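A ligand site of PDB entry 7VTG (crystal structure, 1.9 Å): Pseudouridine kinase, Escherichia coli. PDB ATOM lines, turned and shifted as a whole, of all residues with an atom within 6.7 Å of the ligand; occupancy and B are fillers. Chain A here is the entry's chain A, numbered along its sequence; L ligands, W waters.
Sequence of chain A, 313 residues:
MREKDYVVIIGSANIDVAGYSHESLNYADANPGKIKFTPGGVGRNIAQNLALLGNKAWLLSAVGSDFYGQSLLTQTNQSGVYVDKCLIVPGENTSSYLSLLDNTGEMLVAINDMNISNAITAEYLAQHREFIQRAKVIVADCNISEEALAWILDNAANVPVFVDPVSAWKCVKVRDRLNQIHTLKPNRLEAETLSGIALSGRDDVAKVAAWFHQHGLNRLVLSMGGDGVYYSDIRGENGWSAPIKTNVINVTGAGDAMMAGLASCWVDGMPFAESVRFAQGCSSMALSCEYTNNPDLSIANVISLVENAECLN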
ATOM      1  N   SER A  12     -13.360  24.261 -18.521  1.00  0.00           N
ATOM      2  CA  SER A  12     -12.207  24.973 -18.998  1.00  0.00           C
ATOM      3  C   SER A  12     -12.216  26.467 -18.580  1.00  0.00           C
ATOM      4  O   SER A  12     -13.248  27.098 -18.260  1.00  0.00           O
ATOM      5  CB  SER A  12     -12.086  24.778 -20.512  1.00  0.00           C
ATOM      6  OG  SER A  12     -13.219  25.340 -21.063  1.00  0.00           O
ATOM      7  N   ALA A  13     -10.999  26.979 -18.488  1.00  0.00           N
ATOM      8  CA  ALA A  13     -10.747  28.365 -18.123  1.00  0.00           C
ATOM      9  C   ALA A  13      -9.978  28.999 -19.309  1.00  0.00           C
ATOM     10  O   ALA A  13      -8.862  28.574 -19.629  1.00  0.00           O
ATOM     11  CB  ALA A  13      -9.921  28.437 -16.804  1.00  0.00           C
ATOM     12  N   ASN A  14     -10.638  29.932 -19.981  1.00  0.00           N
ATOM     13  CA  ASN A  14     -10.094  30.591 -21.180  1.00  0.00           C
ATOM     14  C   ASN A  14      -9.748  32.050 -20.927  1.00  0.00           C
ATOM     15  O   ASN A  14     -10.343  32.678 -20.052  1.00  0.00           O
ATOM     16  CB  ASN A  14     -11.097  30.614 -22.332  1.00  0.00           C
ATOM     17  CG  ASN A  14     -11.269  29.297 -23.013  1.00  0.00           C
ATOM     18  OD1 ASN A  14     -10.454  28.369 -22.882  1.00  0.00           O
ATOM     19  ND2 ASN A  14     -12.343  29.214 -23.790  1.00  0.00           N
ATOM     20  N   ILE A  15      -8.877  32.627 -21.765  1.00  0.00           N
ATOM     21  CA  ILE A  15      -8.860  34.088 -21.903  1.00  0.00           C
ATOM     22  C   ILE A  15      -9.552  34.411 -23.183  1.00  0.00           C
ATOM     23  O   ILE A  15      -9.113  33.970 -24.239  1.00  0.00           O
ATOM     24  CB  ILE A  15      -7.416  34.743 -21.925  1.00  0.00           C
ATOM     25  CG1 ILE A  15      -6.622  34.315 -20.690  1.00  0.00           C
ATOM     26  CG2 ILE A  15      -7.535  36.303 -22.065  1.00  0.00           C
ATOM     27  CD1 ILE A  15      -5.166  34.647 -20.752  1.00  0.00           C
ATOM     28  N   ASP A  16     -10.665  35.121 -23.090  1.00  0.00           N
ATOM     29  CA  ASP A  16     -11.314  35.620 -24.261  1.00  0.00           C
ATOM     30  C   ASP A  16     -10.606  36.925 -24.692  1.00  0.00           C
ATOM     31  O   ASP A  16     -10.279  37.754 -23.837  1.00  0.00           O
ATOM     32  CB  ASP A  16     -12.750  35.883 -23.977  1.00  0.00           C
ATOM     33  CG  ASP A  16     -13.522  34.564 -23.697  1.00  0.00           C
ATOM     34  OD1 ASP A  16     -12.890  33.472 -23.776  1.00  0.00           O
ATOM     35  OD2 ASP A  16     -14.739  34.664 -23.447  1.00  0.00           O
ATOM     36  N   THR A  38     -10.740  39.181 -21.388  1.00  0.00           N
ATOM     37  CA  THR A  38     -11.695  38.877 -20.309  1.00  0.00           C
ATOM     38  C   THR A  38     -11.608  37.406 -19.866  1.00  0.00           C
ATOM     39  O   THR A  38     -11.148  36.551 -20.638  1.00  0.00           O
ATOM     40  CB  THR A  38     -13.138  39.179 -20.734  1.00  0.00           C
ATOM     41  OG1 THR A  38     -13.435  38.419 -21.902  1.00  0.00           O
ATOM     42  CG2 THR A  38     -13.318  40.672 -21.062  1.00  0.00           C
ATOM     43  N   PRO A  39     -11.985  37.116 -18.599  1.00  0.00           N
ATOM     44  CA  PRO A  39     -12.056  35.681 -18.277  1.00  0.00           C
ATOM     45  C   PRO A  39     -13.196  34.968 -19.068  1.00  0.00           C
ATOM     46  O   PRO A  39     -14.352  35.441 -19.215  1.00  0.00           O
ATOM     47  CB  PRO A  39     -12.306  35.676 -16.758  1.00  0.00           C
ATOM     48  CG  PRO A  39     -13.012  36.987 -16.488  1.00  0.00           C
ATOM     49  CD  PRO A  39     -12.415  37.970 -17.470  1.00  0.00           C
ATOM     50  N   GLY A  40     -12.867  33.820 -19.636  1.00  0.00           N
ATOM     51  CA  GLY A  40     -13.876  33.014 -20.343  1.00  0.00           C
ATOM     52  C   GLY A  40     -13.760  31.527 -20.032  1.00  0.00           C
ATOM     53  O   GLY A  40     -13.139  31.125 -19.046  1.00  0.00           O
ATOM     54  N   GLY A  41     -14.358  30.689 -20.893  1.00  0.00           N
ATOM     55  CA  GLY A  41     -14.339  29.258 -20.674  1.00  0.00           C
ATOM     56  C   GLY A  41     -15.599  28.874 -19.916  1.00  0.00           C
ATOM     57  O   GLY A  41     -15.854  29.369 -18.829  1.00  0.00           O
ATOM     58  N   VAL A  42     -16.408  27.998 -20.531  1.00  0.00           N
ATOM     59  CA  VAL A  42     -17.700  27.635 -19.964  1.00  0.00           C
ATOM     60  C   VAL A  42     -17.634  27.282 -18.464  1.00  0.00           C
ATOM     61  O   VAL A  42     -18.377  27.865 -17.673  1.00  0.00           O
ATOM     62  CB  VAL A  42     -18.297  26.477 -20.762  1.00  0.00           C
ATOM     63  CG1 VAL A  42     -19.616  25.923 -20.066  1.00  0.00           C
ATOM     64  CG2 VAL A  42     -18.560  26.930 -22.160  1.00  0.00           C
ATOM     65  N   GLY A  43     -16.732  26.377 -18.099  1.00  0.00           N
ATOM     66  CA  GLY A  43     -16.644  25.901 -16.729  1.00  0.00           C
ATOM     67  C   GLY A  43     -16.306  27.039 -15.786  1.00  0.00           C
ATOM     68  O   GLY A  43     -16.989  27.305 -14.810  1.00  0.00           O
ATOM     69  N   ASN A  45     -16.609  30.235 -16.316  1.00  0.00           N
ATOM     70  CA  ASN A  45     -17.719  31.172 -16.242  1.00  0.00           C
ATOM     71  C   ASN A  45     -18.845  30.754 -15.293  1.00  0.00           C
ATOM     72  O   ASN A  45     -19.486  31.592 -14.579  1.00  0.00           O
ATOM     73  CB  ASN A  45     -18.308  31.351 -17.599  1.00  0.00           C
ATOM     74  CG  ASN A  45     -17.333  32.032 -18.578  1.00  0.00           C
ATOM     75  OD1 ASN A  45     -16.212  32.491 -18.206  1.00  0.00           O
ATOM     76  ND2 ASN A  45     -17.762  32.118 -19.842  1.00  0.00           N
ATOM     77  N   SER A  96      -7.493  29.873 -25.061  1.00  0.00           N
ATOM     78  CA  SER A  96      -8.079  31.154 -25.369  1.00  0.00           C
ATOM     79  C   SER A  96      -9.113  31.131 -26.488  1.00  0.00           C
ATOM     80  O   SER A  96      -9.124  30.238 -27.352  1.00  0.00           O
ATOM     81  CB  SER A  96      -6.947  32.170 -25.726  1.00  0.00           C
ATOM     82  OG  SER A  96      -7.546  33.349 -26.265  1.00  0.00           O
ATOM     83  N   TYR A  97     -10.005  32.097 -26.418  1.00  0.00           N
ATOM     84  CA  TYR A  97     -11.016  32.277 -27.424  1.00  0.00           C
ATOM     85  C   TYR A  97     -10.881  33.686 -28.007  1.00  0.00           C
ATOM     86  O   TYR A  97     -11.293  34.696 -27.382  1.00  0.00           O
ATOM     87  CB  TYR A  97     -12.427  32.051 -26.850  1.00  0.00           C
ATOM     88  CG  TYR A  97     -13.461  31.960 -27.914  1.00  0.00           C
ATOM     89  CD1 TYR A  97     -13.554  30.825 -28.706  1.00  0.00           C
ATOM     90  CD2 TYR A  97     -14.319  33.032 -28.183  1.00  0.00           C
ATOM     91  CE1 TYR A  97     -14.496  30.735 -29.727  1.00  0.00           C
ATOM     92  CE2 TYR A  97     -15.270  32.956 -29.219  1.00  0.00           C
ATOM     93  CZ  TYR A  97     -15.346  31.793 -29.982  1.00  0.00           C
ATOM     94  OH  TYR A  97     -16.276  31.673 -31.019  1.00  0.00           O
ATOM     95  N   ASN A 112     -10.192  29.352 -31.885  1.00  0.00           N
ATOM     96  CA  ASN A 112     -10.412  28.546 -30.737  1.00  0.00           C
ATOM     97  C   ASN A 112      -9.159  27.742 -30.380  1.00  0.00           C
ATOM     98  O   ASN A 112      -8.795  26.787 -31.097  1.00  0.00           O
ATOM     99  CB  ASN A 112     -11.584  27.622 -31.028  1.00  0.00           C
ATOM    100  CG  ASN A 112     -11.985  26.871 -29.857  1.00  0.00           C
ATOM    101  OD1 ASN A 112     -11.289  25.946 -29.441  1.00  0.00           O
ATOM    102  ND2 ASN A 112     -13.128  27.222 -29.305  1.00  0.00           N
ATOM    103  N   MET A 114      -7.870  25.533 -27.538  1.00  0.00           N
ATOM    104  CA  MET A 114      -8.174  24.970 -26.231  1.00  0.00           C
ATOM    105  C   MET A 114      -7.527  23.667 -25.924  1.00  0.00           C
ATOM    106  O   MET A 114      -8.111  22.866 -25.199  1.00  0.00           O
ATOM    107  CB  MET A 114      -9.681  24.819 -26.087  1.00  0.00           C
ATOM    108  CG  MET A 114     -10.321  26.156 -26.130  1.00  0.00           C
ATOM    109  SD  MET A 114     -12.034  26.126 -25.705  1.00  0.00           S
ATOM    110  CE  MET A 114     -12.005  25.344 -24.083  1.00  0.00           C
ATOM    111  N   ASP A 141     -18.293  20.644 -17.798  1.00  0.00           N
ATOM    112  CA  ASP A 141     -18.577  21.087 -19.167  1.00  0.00           C
ATOM    113  C   ASP A 141     -18.000  20.060 -20.130  1.00  0.00           C
ATOM    114  O   ASP A 141     -17.164  19.254 -19.714  1.00  0.00           O
ATOM    115  CB  ASP A 141     -18.053  22.538 -19.440  1.00  0.00           C
ATOM    116  CG  ASP A 141     -16.529  22.640 -19.688  1.00  0.00           C
ATOM    117  OD1 ASP A 141     -15.842  21.608 -19.929  1.00  0.00           O
ATOM    118  OD2 ASP A 141     -16.017  23.792 -19.629  1.00  0.00           O
ATOM    119  N   ASN A 143     -15.937  20.543 -22.670  1.00  0.00           N
ATOM    120  CA  ASN A 143     -14.595  20.897 -23.188  1.00  0.00           C
ATOM    121  C   ASN A 143     -13.619  19.819 -22.790  1.00  0.00           C
ATOM    122  O   ASN A 143     -12.601  19.579 -23.473  1.00  0.00           O
ATOM    123  CB  ASN A 143     -14.079  22.233 -22.622  1.00  0.00           C
ATOM    124  CG  ASN A 143     -14.783  23.396 -23.177  1.00  0.00           C
ATOM    125  OD1 ASN A 143     -14.880  23.545 -24.398  1.00  0.00           O
ATOM    126  ND2 ASN A 143     -15.335  24.224 -22.303  1.00  0.00           N
ATOM    127  N   VAL A 166     -21.766  22.542 -24.126  1.00  0.00           N
ATOM    128  CA  VAL A 166     -20.822  23.497 -24.753  1.00  0.00           C
ATOM    129  C   VAL A 166     -21.049  23.829 -26.248  1.00  0.00           C
ATOM    130  O   VAL A 166     -21.152  24.989 -26.589  1.00  0.00           O
ATOM    131  CB  VAL A 166     -19.305  23.058 -24.635  1.00  0.00           C
ATOM    132  CG1 VAL A 166     -18.371  24.082 -25.418  1.00  0.00           C
ATOM    133  CG2 VAL A 166     -18.895  22.951 -23.146  1.00  0.00           C
ATOM    134  N   SER A 167     -21.078  22.824 -27.134  1.00  0.00           N
ATOM    135  CA  SER A 167     -21.249  23.056 -28.602  1.00  0.00           C
ATOM    136  C   SER A 167     -21.788  21.802 -29.272  1.00  0.00           C
ATOM    137  O   SER A 167     -21.792  20.727 -28.659  1.00  0.00           O
ATOM    138  CB  SER A 167     -19.934  23.481 -29.285  1.00  0.00           C
ATOM    139  OG  SER A 167     -18.961  22.430 -29.288  1.00  0.00           O
ATOM    140  N   LYS A 170     -18.895  19.404 -29.371  1.00  0.00           N
ATOM    141  CA  LYS A 170     -18.402  18.826 -28.111  1.00  0.00           C
ATOM    142  C   LYS A 170     -19.496  18.078 -27.340  1.00  0.00           C
ATOM    143  O   LYS A 170     -19.176  17.264 -26.474  1.00  0.00           O
ATOM    144  CB  LYS A 170     -17.783  19.916 -27.236  1.00  0.00           C
ATOM    145  CG  LYS A 170     -16.523  20.409 -27.848  1.00  0.00           C
ATOM    146  CD  LYS A 170     -15.845  21.610 -27.076  1.00  0.00           C
ATOM    147  CE  LYS A 170     -14.611  22.084 -27.866  1.00  0.00           C
ATOM    148  NZ  LYS A 170     -13.671  22.865 -26.956  1.00  0.00           N
ATOM    149  N   VAL A 251     -24.730  38.369 -25.883  1.00  0.00           N
ATOM    150  CA  VAL A 251     -25.287  37.031 -25.731  1.00  0.00           C
ATOM    151  C   VAL A 251     -24.286  36.028 -25.129  1.00  0.00           C
ATOM    152  O   VAL A 251     -24.681  34.993 -24.561  1.00  0.00           O
ATOM    153  CB  VAL A 251     -25.763  36.523 -27.091  1.00  0.00           C
ATOM    154  CG1 VAL A 251     -26.768  37.501 -27.661  1.00  0.00           C
ATOM    155  CG2 VAL A 251     -24.579  36.338 -28.032  1.00  0.00           C
ATOM    156  N   THR A 252     -23.005  36.338 -25.218  1.00  0.00           N
ATOM    157  CA  THR A 252     -21.969  35.537 -24.605  1.00  0.00           C
ATOM    158  C   THR A 252     -22.222  35.459 -23.101  1.00  0.00           C
ATOM    159  O   THR A 252     -22.424  36.489 -22.418  1.00  0.00           O
ATOM    160  CB  THR A 252     -20.578  36.112 -24.834  1.00  0.00           C
ATOM    161  OG1 THR A 252     -20.385  36.382 -26.229  1.00  0.00           O
ATOM    162  CG2 THR A 252     -19.496  35.163 -24.308  1.00  0.00           C
ATOM    163  N   GLY A 253     -22.195  34.238 -22.585  1.00  0.00           N
ATOM    164  CA  GLY A 253     -22.398  34.076 -21.136  1.00  0.00           C
ATOM    165  C   GLY A 253     -23.835  33.759 -20.675  1.00  0.00           C
ATOM    166  O   GLY A 253     -24.045  33.463 -19.484  1.00  0.00           O
ATOM    167  N   ALA A 254     -24.803  33.818 -21.586  1.00  0.00           N
ATOM    168  CA  ALA A 254     -26.212  33.583 -21.230  1.00  0.00           C
ATOM    169  C   ALA A 254     -26.445  32.138 -20.751  1.00  0.00           C
ATOM    170  O   ALA A 254     -27.108  31.912 -19.733  1.00  0.00           O
ATOM    171  CB  ALA A 254     -27.119  33.890 -22.422  1.00  0.00           C
ATOM    172  N   GLY A 255     -25.865  31.181 -21.489  1.00  0.00           N
ATOM    173  CA  GLY A 255     -25.988  29.768 -21.178  1.00  0.00           C
ATOM    174  C   GLY A 255     -25.262  29.442 -19.866  1.00  0.00           C
ATOM    175  O   GLY A 255     -25.718  28.582 -19.096  1.00  0.00           O
ATOM    176  N   ASP A 256     -24.150  30.145 -19.617  1.00  0.00           N
ATOM    177  CA  ASP A 256     -23.334  29.926 -18.423  1.00  0.00           C
ATOM    178  C   ASP A 256     -24.024  30.418 -17.154  1.00  0.00           C
ATOM    179  O   ASP A 256     -23.876  29.804 -16.090  1.00  0.00           O
ATOM    180  CB  ASP A 256     -21.961  30.599 -18.534  1.00  0.00           C
ATOM    181  CG  ASP A 256     -21.151  30.049 -19.714  1.00  0.00           C
ATOM    182  OD1 ASP A 256     -21.332  28.862 -20.071  1.00  0.00           O
ATOM    183  OD2 ASP A 256     -20.322  30.791 -20.276  1.00  0.00           O
ATOM    184  N   THR A 292     -19.085  38.741 -20.200  1.00  0.00           N
ATOM    185  CA  THR A 292     -19.372  37.330 -20.307  1.00  0.00           C
ATOM    186  C   THR A 292     -20.039  36.894 -18.957  1.00  0.00           C
ATOM    187  O   THR A 292     -20.909  36.015 -18.911  1.00  0.00           O
ATOM    188  CB  THR A 292     -18.080  36.522 -20.591  1.00  0.00           C
ATOM    189  OG1 THR A 292     -17.332  37.122 -21.670  1.00  0.00           O
ATOM    190  CG2 THR A 292     -18.403  35.069 -20.897  1.00  0.00           C
HETATM  191  O1  LIG L   1     -15.197  25.265 -27.464  1.00  0.00           O
HETATM  192  C1  LIG L   1     -15.366  26.247 -26.738  1.00  0.00           C
HETATM  193  N1  LIG L   1     -15.584  27.603 -27.235  1.00  0.00           N
HETATM  194  C2  LIG L   1     -15.778  28.730 -26.391  1.00  0.00           C
HETATM  195  C3  LIG L   1     -15.720  28.545 -24.940  1.00  0.00           C
HETATM  196  C4  LIG L   1     -15.514  27.169 -24.409  1.00  0.00           C
HETATM  197  O2  LIG L   1     -15.445  26.971 -23.212  1.00  0.00           O
HETATM  198  N2  LIG L   1     -15.310  26.079 -25.290  1.00  0.00           N
HETATM  199  C5  LIG L   1     -15.943  29.692 -23.974  1.00  0.00           C
HETATM  200  O3  LIG L   1     -17.465  29.838 -23.959  1.00  0.00           O
HETATM  201  C6  LIG L   1     -17.605  31.211 -23.206  1.00  0.00           C
HETATM  202  C7  LIG L   1     -19.114  31.605 -23.359  1.00  0.00           C
HETATM  203  O4  LIG L   1     -19.961  30.524 -22.955  1.00  0.00           O
HETATM  204  C8  LIG L   1     -16.688  31.935 -23.736  1.00  0.00           C
HETATM  205  O5  LIG L   1     -15.993  32.521 -22.602  1.00  0.00           O
HETATM  206  C9  LIG L   1     -15.534  30.880 -24.364  1.00  0.00           C
HETATM  207  O6  LIG L   1     -14.243  31.098 -23.783  1.00  0.00           O
HETATM  208  O   HOH W   1     -15.911  27.862 -30.174  1.00  0.00           O
HETATM  209  O   HOH W   2     -23.075  31.215 -22.253  1.00  0.00           O
HETATM  210  O   HOH W   3     -16.738  23.711 -29.975  1.00  0.00           O
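N of Gly 40 lies within hydrogen-bond range of O of Asn 14 (2.8 Å).
ND2 of Asn 14 sits at hydrogen-bond distance from SD of Met 114 (3.6 Å).
The side-chain carboxylate (OD2) of Asp 256 sits at hydrogen-bond distance from the side-chain amide nitrogen (ND2) of Asn 45.
OD2 of Asp 141 lies within hydrogen-bond range of ND2 of Asn 143, 2.8 Å away.
OD1 of Asn 45 sits close to O of Gly 41 (3.2 Å).
OD1 of Asn 45 lies close to O of Gly 40 (3.5 Å).
The side-chain carboxylate (OD2) of Asp 141 is in hydrogen-bond range of the backbone NH (N) of Ser 12.
N of Tyr 97 lies within hydrogen-bond range of O of Ile 15 (3.0 Å).
Residues that only touch the ligand: Gly 40 (3.1 Å), Tyr 97 (3.7 Å), Val 166 (3.7 Å), Thr 252 (3.7 Å) and Thr 292 (3.9 Å).
Hydrophobic or aromatic side chains that line the ligand: Val 42, Tyr 97, Met 114 and Val 166.
Of the 28 residues printed, 16 come within 4 Å of the ligand.
The side-chain carboxylate of Asp 16 is in hydrogen-bond range of an oxygen (O5) of the ligand (2.6 Å).
O6 of the ligand is in hydrogen-bond range of ND2 of Asn 14 (2.7 Å).
The side-chain carboxylate (OD2) of Asp 256 is in hydrogen-bond range of an oxygen (O4) of the ligand, 2.7 Å away.
The side-chain amide oxygen (OD1) of Asn 143 sits at hydrogen-bond distance from a nitrogen (N2) of the ligand (2.7 Å).
An oxygen (O1) of the ligand lies within hydrogen-bond range of the side-chain amino group (NZ) of Lys 170 (2.9 Å).
An oxygen (O6) of the ligand is in hydrogen-bond range of the backbone NH (N) of Gly 41 (2.9 Å).
The backbone NH (N) of Val 42 lies within hydrogen-bond range of an oxygen (O2) of the ligand (3.0 Å).
The side-chain amide nitrogen of Asn 112 lies close to a nitrogen (N1) of the ligand.
The side-chain sulfur of Met 114 sits at hydrogen-bond distance from a nitrogen (N2) of the ligand.
O5 of the ligand is in hydrogen-bond range of ND2 of Asn 45 (3.3 Å).
An oxygen (O2) of the ligand sits at hydrogen-bond distance from the side-chain hydroxyl of Ser 12 (3.5 Å).
Water W1 lies within hydrogen-bond range of N1 of the ligand and ND2 of Asn 112.
Water W3 lies within hydrogen-bond range of OG of Ser 167 (2.7 Å) and O1 of the ligand (3.3 Å).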
